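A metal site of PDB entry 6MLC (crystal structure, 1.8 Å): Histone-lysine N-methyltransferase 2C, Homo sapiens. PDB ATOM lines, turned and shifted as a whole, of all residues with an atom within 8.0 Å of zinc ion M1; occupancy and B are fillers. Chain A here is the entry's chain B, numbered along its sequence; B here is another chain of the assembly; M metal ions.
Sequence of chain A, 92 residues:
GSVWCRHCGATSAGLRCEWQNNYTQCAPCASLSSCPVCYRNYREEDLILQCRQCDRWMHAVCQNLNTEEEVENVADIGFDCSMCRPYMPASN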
ATOM      1  N   CYS A   5     -14.094  -0.926  12.819  1.00  0.00           N
ATOM      2  CA  CYS A   5     -13.281  -1.656  11.837  1.00  0.00           C
ATOM      3  C   CYS A   5     -12.757  -2.943  12.469  1.00  0.00           C
ATOM      4  O   CYS A   5     -11.863  -2.882  13.314  1.00  0.00           O
ATOM      5  CB  CYS A   5     -12.121  -0.815  11.354  1.00  0.00           C
ATOM      6  SG  CYS A   5     -11.194  -1.698  10.086  1.00  0.00           S
ATOM      7  N   HIS A   7     -10.932  -5.066  11.032  1.00  0.00           N
ATOM      8  CA  HIS A   7      -9.559  -5.263  10.518  1.00  0.00           C
ATOM      9  C   HIS A   7      -8.492  -4.739  11.478  1.00  0.00           C
ATOM     10  O   HIS A   7      -7.377  -5.328  11.500  1.00  0.00           O
ATOM     11  CB  HIS A   7      -9.383  -4.611   9.140  1.00  0.00           C
ATOM     12  CG  HIS A   7     -10.271  -5.139   8.060  1.00  0.00           C
ATOM     13  ND1 HIS A   7     -10.039  -6.385   7.423  1.00  0.00           N
ATOM     14  CD2 HIS A   7     -11.308  -4.555   7.414  1.00  0.00           C
ATOM     15  CE1 HIS A   7     -10.934  -6.550   6.494  1.00  0.00           C
ATOM     16  NE2 HIS A   7     -11.737  -5.427   6.459  1.00  0.00           N
ATOM     17  N   LEU A  15     -14.852   5.410   6.377  1.00  0.00           N
ATOM     18  CA  LEU A  15     -14.369   5.882   5.047  1.00  0.00           C
ATOM     19  C   LEU A  15     -14.220   4.683   4.106  1.00  0.00           C
ATOM     20  O   LEU A  15     -14.033   3.567   4.606  1.00  0.00           O
ATOM     21  CB  LEU A  15     -13.050   6.638   5.231  1.00  0.00           C
ATOM     22  CG  LEU A  15     -13.046   7.661   6.374  1.00  0.00           C
ATOM     23  CD1 LEU A  15     -11.693   8.348   6.472  1.00  0.00           C
ATOM     24  CD2 LEU A  15     -14.168   8.677   6.197  1.00  0.00           C
ATOM     25  N   ARG A  16     -14.423   4.934   2.822  1.00  0.00           N
ATOM     26  CA  ARG A  16     -14.182   3.963   1.720  1.00  0.00           C
ATOM     27  C   ARG A  16     -12.858   3.220   1.999  1.00  0.00           C
ATOM     28  O   ARG A  16     -11.865   3.878   2.170  1.00  0.00           O
ATOM     29  CB  ARG A  16     -14.153   4.715   0.389  1.00  0.00           C
ATOM     30  CG  ARG A  16     -13.613   3.922  -0.799  1.00  0.00           C
ATOM     31  CD  ARG A  16     -13.832   4.649  -2.126  1.00  0.00           C
ATOM     32  NE  ARG A  16     -13.378   3.829  -3.238  1.00  0.00           N
ATOM     33  CZ  ARG A  16     -14.154   2.973  -3.890  1.00  0.00           C
ATOM     34  NH1 ARG A  16     -15.428   2.841  -3.563  1.00  0.00           N
ATOM     35  NH2 ARG A  16     -13.654   2.247  -4.880  1.00  0.00           N
ATOM     36  N   CYS A  17     -12.880   1.894   1.999  1.00  0.00           N
ATOM     37  CA  CYS A  17     -11.625   1.099   2.002  1.00  0.00           C
ATOM     38  C   CYS A  17     -10.743   1.526   0.830  1.00  0.00           C
ATOM     39  O   CYS A  17     -11.270   1.644  -0.297  1.00  0.00           O
ATOM     40  CB  CYS A  17     -11.947  -0.395   1.892  1.00  0.00           C
ATOM     41  SG  CYS A  17     -10.470  -1.437   1.831  1.00  0.00           S
ATOM     42  N   GLU A  18      -9.451   1.734   1.084  1.00  0.00           N
ATOM     43  CA  GLU A  18      -8.416   2.020   0.068  1.00  0.00           C
ATOM     44  C   GLU A  18      -7.263   1.033   0.194  1.00  0.00           C
ATOM     45  O   GLU A  18      -6.132   1.364  -0.175  1.00  0.00           O
ATOM     46  CB  GLU A  18      -7.907   3.455   0.242  1.00  0.00           C
ATOM     47  CG  GLU A  18      -8.995   4.461   0.039  1.00  0.00           C
ATOM     48  CD  GLU A  18      -8.503   5.893  -0.025  1.00  0.00           C
ATOM     49  OE1 GLU A  18      -7.377   6.170   0.453  1.00  0.00           O
ATOM     50  OE2 GLU A  18      -9.264   6.722  -0.535  1.00  0.00           O
ATOM     51  N   TRP A  19      -7.555  -0.165   0.701  1.00  0.00           N
ATOM     52  CA  TRP A  19      -6.550  -1.226   0.934  1.00  0.00           C
ATOM     53  C   TRP A  19      -5.908  -1.606  -0.395  1.00  0.00           C
ATOM     54  O   TRP A  19      -4.697  -1.866  -0.407  1.00  0.00           O
ATOM     55  CB  TRP A  19      -7.188  -2.447   1.566  1.00  0.00           C
ATOM     56  CG  TRP A  19      -6.289  -3.626   1.663  1.00  0.00           C
ATOM     57  CD1 TRP A  19      -6.115  -4.612   0.730  1.00  0.00           C
ATOM     58  CD2 TRP A  19      -5.440  -3.959   2.764  1.00  0.00           C
ATOM     59  NE1 TRP A  19      -5.227  -5.540   1.191  1.00  0.00           N
ATOM     60  CE2 TRP A  19      -4.812  -5.184   2.437  1.00  0.00           C
ATOM     61  CE3 TRP A  19      -5.157  -3.369   4.005  1.00  0.00           C
ATOM     62  CZ2 TRP A  19      -3.910  -5.798   3.286  1.00  0.00           C
ATOM     63  CZ3 TRP A  19      -4.300  -4.006   4.863  1.00  0.00           C
ATOM     64  CH2 TRP A  19      -3.661  -5.189   4.489  1.00  0.00           C
ATOM     65  N   GLN A  20      -6.730  -1.788  -1.424  1.00  0.00           N
ATOM     66  CA  GLN A  20      -6.190  -2.161  -2.745  1.00  0.00           C
ATOM     67  C   GLN A  20      -5.495  -0.922  -3.333  1.00  0.00           C
ATOM     68  O   GLN A  20      -4.258  -0.937  -3.456  1.00  0.00           O
ATOM     69  CB  GLN A  20      -7.273  -2.792  -3.617  1.00  0.00           C
ATOM     70  CG  GLN A  20      -6.769  -3.190  -5.000  1.00  0.00           C
ATOM     71  CD  GLN A  20      -5.577  -4.113  -4.952  1.00  0.00           C
ATOM     72  OE1 GLN A  20      -4.517  -3.795  -5.470  1.00  0.00           O
ATOM     73  NE2 GLN A  20      -5.734  -5.265  -4.283  1.00  0.00           N
ATOM     74  N   THR A  24      -9.955   1.633  -5.234  1.00  0.00           N
ATOM     75  CA  THR A  24     -10.368   0.228  -5.125  1.00  0.00           C
ATOM     76  C   THR A  24     -10.398  -0.206  -3.654  1.00  0.00           C
ATOM     77  O   THR A  24      -9.351  -0.207  -3.005  1.00  0.00           O
ATOM     78  CB  THR A  24      -9.469  -0.659  -5.988  1.00  0.00           C
ATOM     79  OG1 THR A  24      -9.167   0.097  -7.164  1.00  0.00           O
ATOM     80  CG2 THR A  24     -10.112  -1.977  -6.330  1.00  0.00           C
ATOM     81  N   GLN A  25     -11.587  -0.577  -3.204  1.00  0.00           N
ATOM     82  CA  GLN A  25     -11.819  -1.308  -1.932  1.00  0.00           C
ATOM     83  C   GLN A  25     -11.239  -2.713  -2.080  1.00  0.00           C
ATOM     84  O   GLN A  25     -11.237  -3.266  -3.211  1.00  0.00           O
ATOM     85  CB  GLN A  25     -13.332  -1.347  -1.629  1.00  0.00           C
ATOM     86  CG  GLN A  25     -13.957   0.035  -1.544  1.00  0.00           C
ATOM     87  CD  GLN A  25     -15.148   0.045  -0.607  1.00  0.00           C
ATOM     88  OE1 GLN A  25     -15.048   0.476   0.557  1.00  0.00           O
ATOM     89  NE2 GLN A  25     -16.276  -0.429  -1.103  1.00  0.00           N
ATOM     90  N   CYS A  26     -10.797  -3.304  -0.985  1.00  0.00           N
ATOM     91  CA  CYS A  26     -10.530  -4.752  -0.970  1.00  0.00           C
ATOM     92  C   CYS A  26     -11.881  -5.454  -1.167  1.00  0.00           C
ATOM     93  O   CYS A  26     -12.919  -4.835  -0.919  1.00  0.00           O
ATOM     94  CB  CYS A  26      -9.768  -5.202   0.284  1.00  0.00           C
ATOM     95  SG  CYS A  26     -10.717  -5.267   1.814  1.00  0.00           S
ATOM     96  N   ALA A  27     -11.881  -6.663  -1.716  1.00  0.00           N
ATOM     97  CA  ALA A  27     -13.149  -7.371  -2.004  1.00  0.00           C
ATOM     98  C   ALA A  27     -13.924  -7.611  -0.708  1.00  0.00           C
ATOM     99  O   ALA A  27     -15.147  -7.463  -0.709  1.00  0.00           O
ATOM    100  CB  ALA A  27     -12.892  -8.651  -2.775  1.00  0.00           C
ATOM    101  N   PRO A  28     -13.298  -7.999   0.415  1.00  0.00           N
ATOM    102  CA  PRO A  28     -14.031  -8.178   1.685  1.00  0.00           C
ATOM    103  C   PRO A  28     -14.783  -6.915   2.133  1.00  0.00           C
ATOM    104  O   PRO A  28     -15.983  -7.018   2.393  1.00  0.00           O
ATOM    105  CB  PRO A  28     -12.922  -8.630   2.654  1.00  0.00           C
ATOM    106  CG  PRO A  28     -11.931  -9.324   1.739  1.00  0.00           C
ATOM    107  CD  PRO A  28     -11.889  -8.401   0.533  1.00  0.00           C
ATOM    108  N   CYS A  29     -14.148  -5.754   2.114  1.00  0.00           N
ATOM    109  CA  CYS A  29     -14.808  -4.463   2.507  1.00  0.00           C
ATOM    110  C   CYS A  29     -15.964  -4.145   1.545  1.00  0.00           C
ATOM    111  O   CYS A  29     -17.045  -3.841   2.036  1.00  0.00           O
ATOM    112  CB  CYS A  29     -13.821  -3.307   2.582  1.00  0.00           C
ATOM    113  SG  CYS A  29     -12.803  -3.388   4.079  1.00  0.00           S
ATOM    114  N   ALA A  30     -15.761  -4.276   0.223  1.00  0.00           N
ATOM    115  CA  ALA A  30     -16.839  -4.016  -0.770  1.00  0.00           C
ATOM    116  C   ALA A  30     -18.042  -4.919  -0.466  1.00  0.00           C
ATOM    117  O   ALA A  30     -19.184  -4.459  -0.622  1.00  0.00           O
ATOM    118  CB  ALA A  30     -16.325  -4.205  -2.178  1.00  0.00           C
ATOM    119  N   LEU A  32     -19.335  -5.886   2.189  1.00  0.00           N
ATOM    120  CA  LEU A  32     -20.175  -5.435   3.328  1.00  0.00           C
ATOM    121  C   LEU A  32     -21.444  -4.778   2.805  1.00  0.00           C
ATOM    122  O   LEU A  32     -22.472  -4.915   3.470  1.00  0.00           O
ATOM    123  CB  LEU A  32     -19.421  -4.431   4.188  1.00  0.00           C
ATOM    124  CG  LEU A  32     -18.397  -5.005   5.147  1.00  0.00           C
ATOM    125  CD1 LEU A  32     -17.586  -3.880   5.788  1.00  0.00           C
ATOM    126  CD2 LEU A  32     -19.084  -5.866   6.212  1.00  0.00           C
ATOM    127  N   CYS B   5      -5.101   2.826   9.183  1.00  0.00           N
ATOM    128  CA  CYS B   5      -5.664   1.597   8.569  1.00  0.00           C
ATOM    129  C   CYS B   5      -6.237   1.950   7.192  1.00  0.00           C
ATOM    130  O   CYS B   5      -7.130   2.818   7.139  1.00  0.00           O
ATOM    131  CB  CYS B   5      -6.710   1.010   9.472  1.00  0.00           C
ATOM    132  SG  CYS B   5      -7.595  -0.370   8.702  1.00  0.00           S
ATOM    133  N   ARG B   6      -5.809   1.282   6.112  1.00  0.00           N
ATOM    134  CA  ARG B   6      -6.261   1.637   4.739  1.00  0.00           C
ATOM    135  C   ARG B   6      -7.681   1.119   4.543  1.00  0.00           C
ATOM    136  O   ARG B   6      -8.397   1.664   3.687  1.00  0.00           O
ATOM    137  CB  ARG B   6      -5.276   1.136   3.678  1.00  0.00           C
ATOM    138  CG  ARG B   6      -3.890   1.758   3.781  1.00  0.00           C
ATOM    139  CD  ARG B   6      -3.881   3.273   3.604  1.00  0.00           C
ATOM    140  N   HIS B   7      -8.139   0.200   5.380  1.00  0.00           N
ATOM    141  CA  HIS B   7      -9.505  -0.341   5.286  1.00  0.00           C
ATOM    142  C   HIS B   7     -10.525   0.701   5.709  1.00  0.00           C
ATOM    143  O   HIS B   7     -11.590   0.738   5.072  1.00  0.00           O
ATOM    144  CB  HIS B   7      -9.691  -1.604   6.134  1.00  0.00           C
ATOM    145  CG  HIS B   7      -8.957  -2.807   5.653  1.00  0.00           C
ATOM    146  ND1 HIS B   7      -9.289  -3.494   4.464  1.00  0.00           N
ATOM    147  CD2 HIS B   7      -7.941  -3.505   6.203  1.00  0.00           C
ATOM    148  CE1 HIS B   7      -8.563  -4.565   4.368  1.00  0.00           C
ATOM    149  NE2 HIS B   7      -7.711  -4.609   5.419  1.00  0.00           N
ATOM    150  N   CYS B   8     -10.296   1.405   6.852  1.00  0.00           N
ATOM    151  CA  CYS B   8     -11.326   2.287   7.485  1.00  0.00           C
ATOM    152  C   CYS B   8     -10.899   3.756   7.408  1.00  0.00           C
ATOM    153  O   CYS B   8     -11.772   4.625   7.643  1.00  0.00           O
ATOM    154  CB  CYS B   8     -11.621   1.920   8.943  1.00  0.00           C
ATOM    155  SG  CYS B   8     -10.176   2.020  10.032  1.00  0.00           S
ATOM    156  N   TRP B  19     -11.875 -10.022  11.277  1.00  0.00           N
ATOM    157  CA  TRP B  19     -12.861  -9.977  10.168  1.00  0.00           C
ATOM    158  C   TRP B  19     -13.550 -11.327   9.979  1.00  0.00           C
ATOM    159  O   TRP B  19     -14.770 -11.338   9.812  1.00  0.00           O
ATOM    160  CB  TRP B  19     -12.159  -9.571   8.886  1.00  0.00           C
ATOM    161  CG  TRP B  19     -13.046  -9.564   7.694  1.00  0.00           C
ATOM    162  CD1 TRP B  19     -13.259 -10.579   6.810  1.00  0.00           C
ATOM    163  CD2 TRP B  19     -13.842  -8.466   7.235  1.00  0.00           C
ATOM    164  NE1 TRP B  19     -14.166 -10.204   5.859  1.00  0.00           N
ATOM    165  CE2 TRP B  19     -14.500  -8.888   6.062  1.00  0.00           C
ATOM    166  CE3 TRP B  19     -14.050  -7.161   7.681  1.00  0.00           C
ATOM    167  CZ2 TRP B  19     -15.364  -8.053   5.354  1.00  0.00           C
ATOM    168  CZ3 TRP B  19     -14.851  -6.327   6.960  1.00  0.00           C
ATOM    169  CH2 TRP B  19     -15.552  -6.786   5.839  1.00  0.00           C
ATOM    170  N   CYS B  26      -8.690 -11.766   8.204  1.00  0.00           N
ATOM    171  CA  CYS B  26      -8.886 -11.923   6.735  1.00  0.00           C
ATOM    172  C   CYS B  26      -7.518 -12.198   6.111  1.00  0.00           C
ATOM    173  O   CYS B  26      -6.443 -11.840   6.732  1.00  0.00           O
ATOM    174  CB  CYS B  26      -9.604 -10.742   6.088  1.00  0.00           C
ATOM    175  SG  CYS B  26      -8.626  -9.238   5.959  1.00  0.00           S
ATOM    176  N   PRO B  28      -6.125 -10.907   3.463  1.00  0.00           N
ATOM    177  CA  PRO B  28      -5.408  -9.645   3.171  1.00  0.00           C
ATOM    178  C   PRO B  28      -4.624  -9.074   4.374  1.00  0.00           C
ATOM    179  O   PRO B  28      -3.431  -8.844   4.204  1.00  0.00           O
ATOM    180  CB  PRO B  28      -6.551  -8.733   2.702  1.00  0.00           C
ATOM    181  CG  PRO B  28      -7.466  -9.711   1.991  1.00  0.00           C
ATOM    182  CD  PRO B  28      -7.524 -10.872   2.960  1.00  0.00           C
ATOM    183  N   CYS B  29      -5.254  -8.944   5.552  1.00  0.00           N
ATOM    184  CA  CYS B  29      -4.592  -8.480   6.800  1.00  0.00           C
ATOM    185  C   CYS B  29      -3.465  -9.429   7.213  1.00  0.00           C
ATOM    186  O   CYS B  29      -2.394  -8.931   7.482  1.00  0.00           O
ATOM    187  CB  CYS B  29      -5.576  -8.284   7.945  1.00  0.00           C
ATOM    188  SG  CYS B  29      -6.652  -6.862   7.662  1.00  0.00           S
ATOM    189  N   ASP B  55      -6.103  -9.366  -3.113  1.00  0.00           N
ATOM    190  CA  ASP B  55      -5.814  -8.205  -2.204  1.00  0.00           C
ATOM    191  C   ASP B  55      -4.697  -8.552  -1.212  1.00  0.00           C
ATOM    192  O   ASP B  55      -4.520  -7.816  -0.244  1.00  0.00           O
ATOM    193  CB  ASP B  55      -7.064  -7.734  -1.456  1.00  0.00           C
ATOM    194  CG  ASP B  55      -8.207  -7.353  -2.386  1.00  0.00           C
ATOM    195  OD1 ASP B  55      -7.948  -6.607  -3.341  1.00  0.00           O
ATOM    196  OD2 ASP B  55      -9.326  -7.830  -2.165  1.00  0.00           O
HETATM  197 ZN    ZN M   1     -10.785  -3.332   3.038  1.00  0.00          ZN
HETATM  198 ZN    ZN M   2      -8.630  -7.857   7.826  1.00  0.00          ZN
HETATM  199 ZN    ZN M   3      -9.408  -0.131  10.198  1.00  0.00          ZN
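Zinc ion M1 is bound by ND1 of His 7 of chain B (2.1 Å).
The side-chain sulfur (SG) of Cys 17 is bound to zinc ion M1 (2.3 Å).
Zinc ion M1 is bound by the side-chain sulfur (SG) of Cys 29 of chain A.
SG of Cys 26 of chain A binds zinc ion M1 (2.3 Å).
Zinc ion M1 has four donor atoms within binding distance.
A ring nitrogen (NE2) of His 7 of chain B sits close to the side-chain sulfur of Cys 29 of chain B (3.4 Å).
N of His 7 of chain B sits close to SG of Cys 5 of chain B (3.4 Å).
SG of Cys 17 sits close to N of Trp 19 of chain A, 3.4 Å away.
The backbone NH of Cys 17 sits at hydrogen-bond distance from the side-chain amide oxygen of Gln 25, at 3.0 Å.
The side-chain sulfur (SG) of Cys 29 of chain A sits close to a ring nitrogen (NE2) of His 7 of chain A.
The indole nitrogen (NE1) of Trp 19 of chain A lies within hydrogen-bond range of the backbone carbonyl oxygen (O) of Asp 55 of chain B.
Trp 19 of chain A touches zinc ion M1 (CB to ZN, 3.99 Å).
Within 4 Å of zinc ion M1: Cys 17, Trp 19 of chain A, Cys 26 of chain A, Cys 29 of chain A and His 7 of chain B.
Along chain A the residues within 4 Å of zinc ion M1 span positions 17 to 29.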
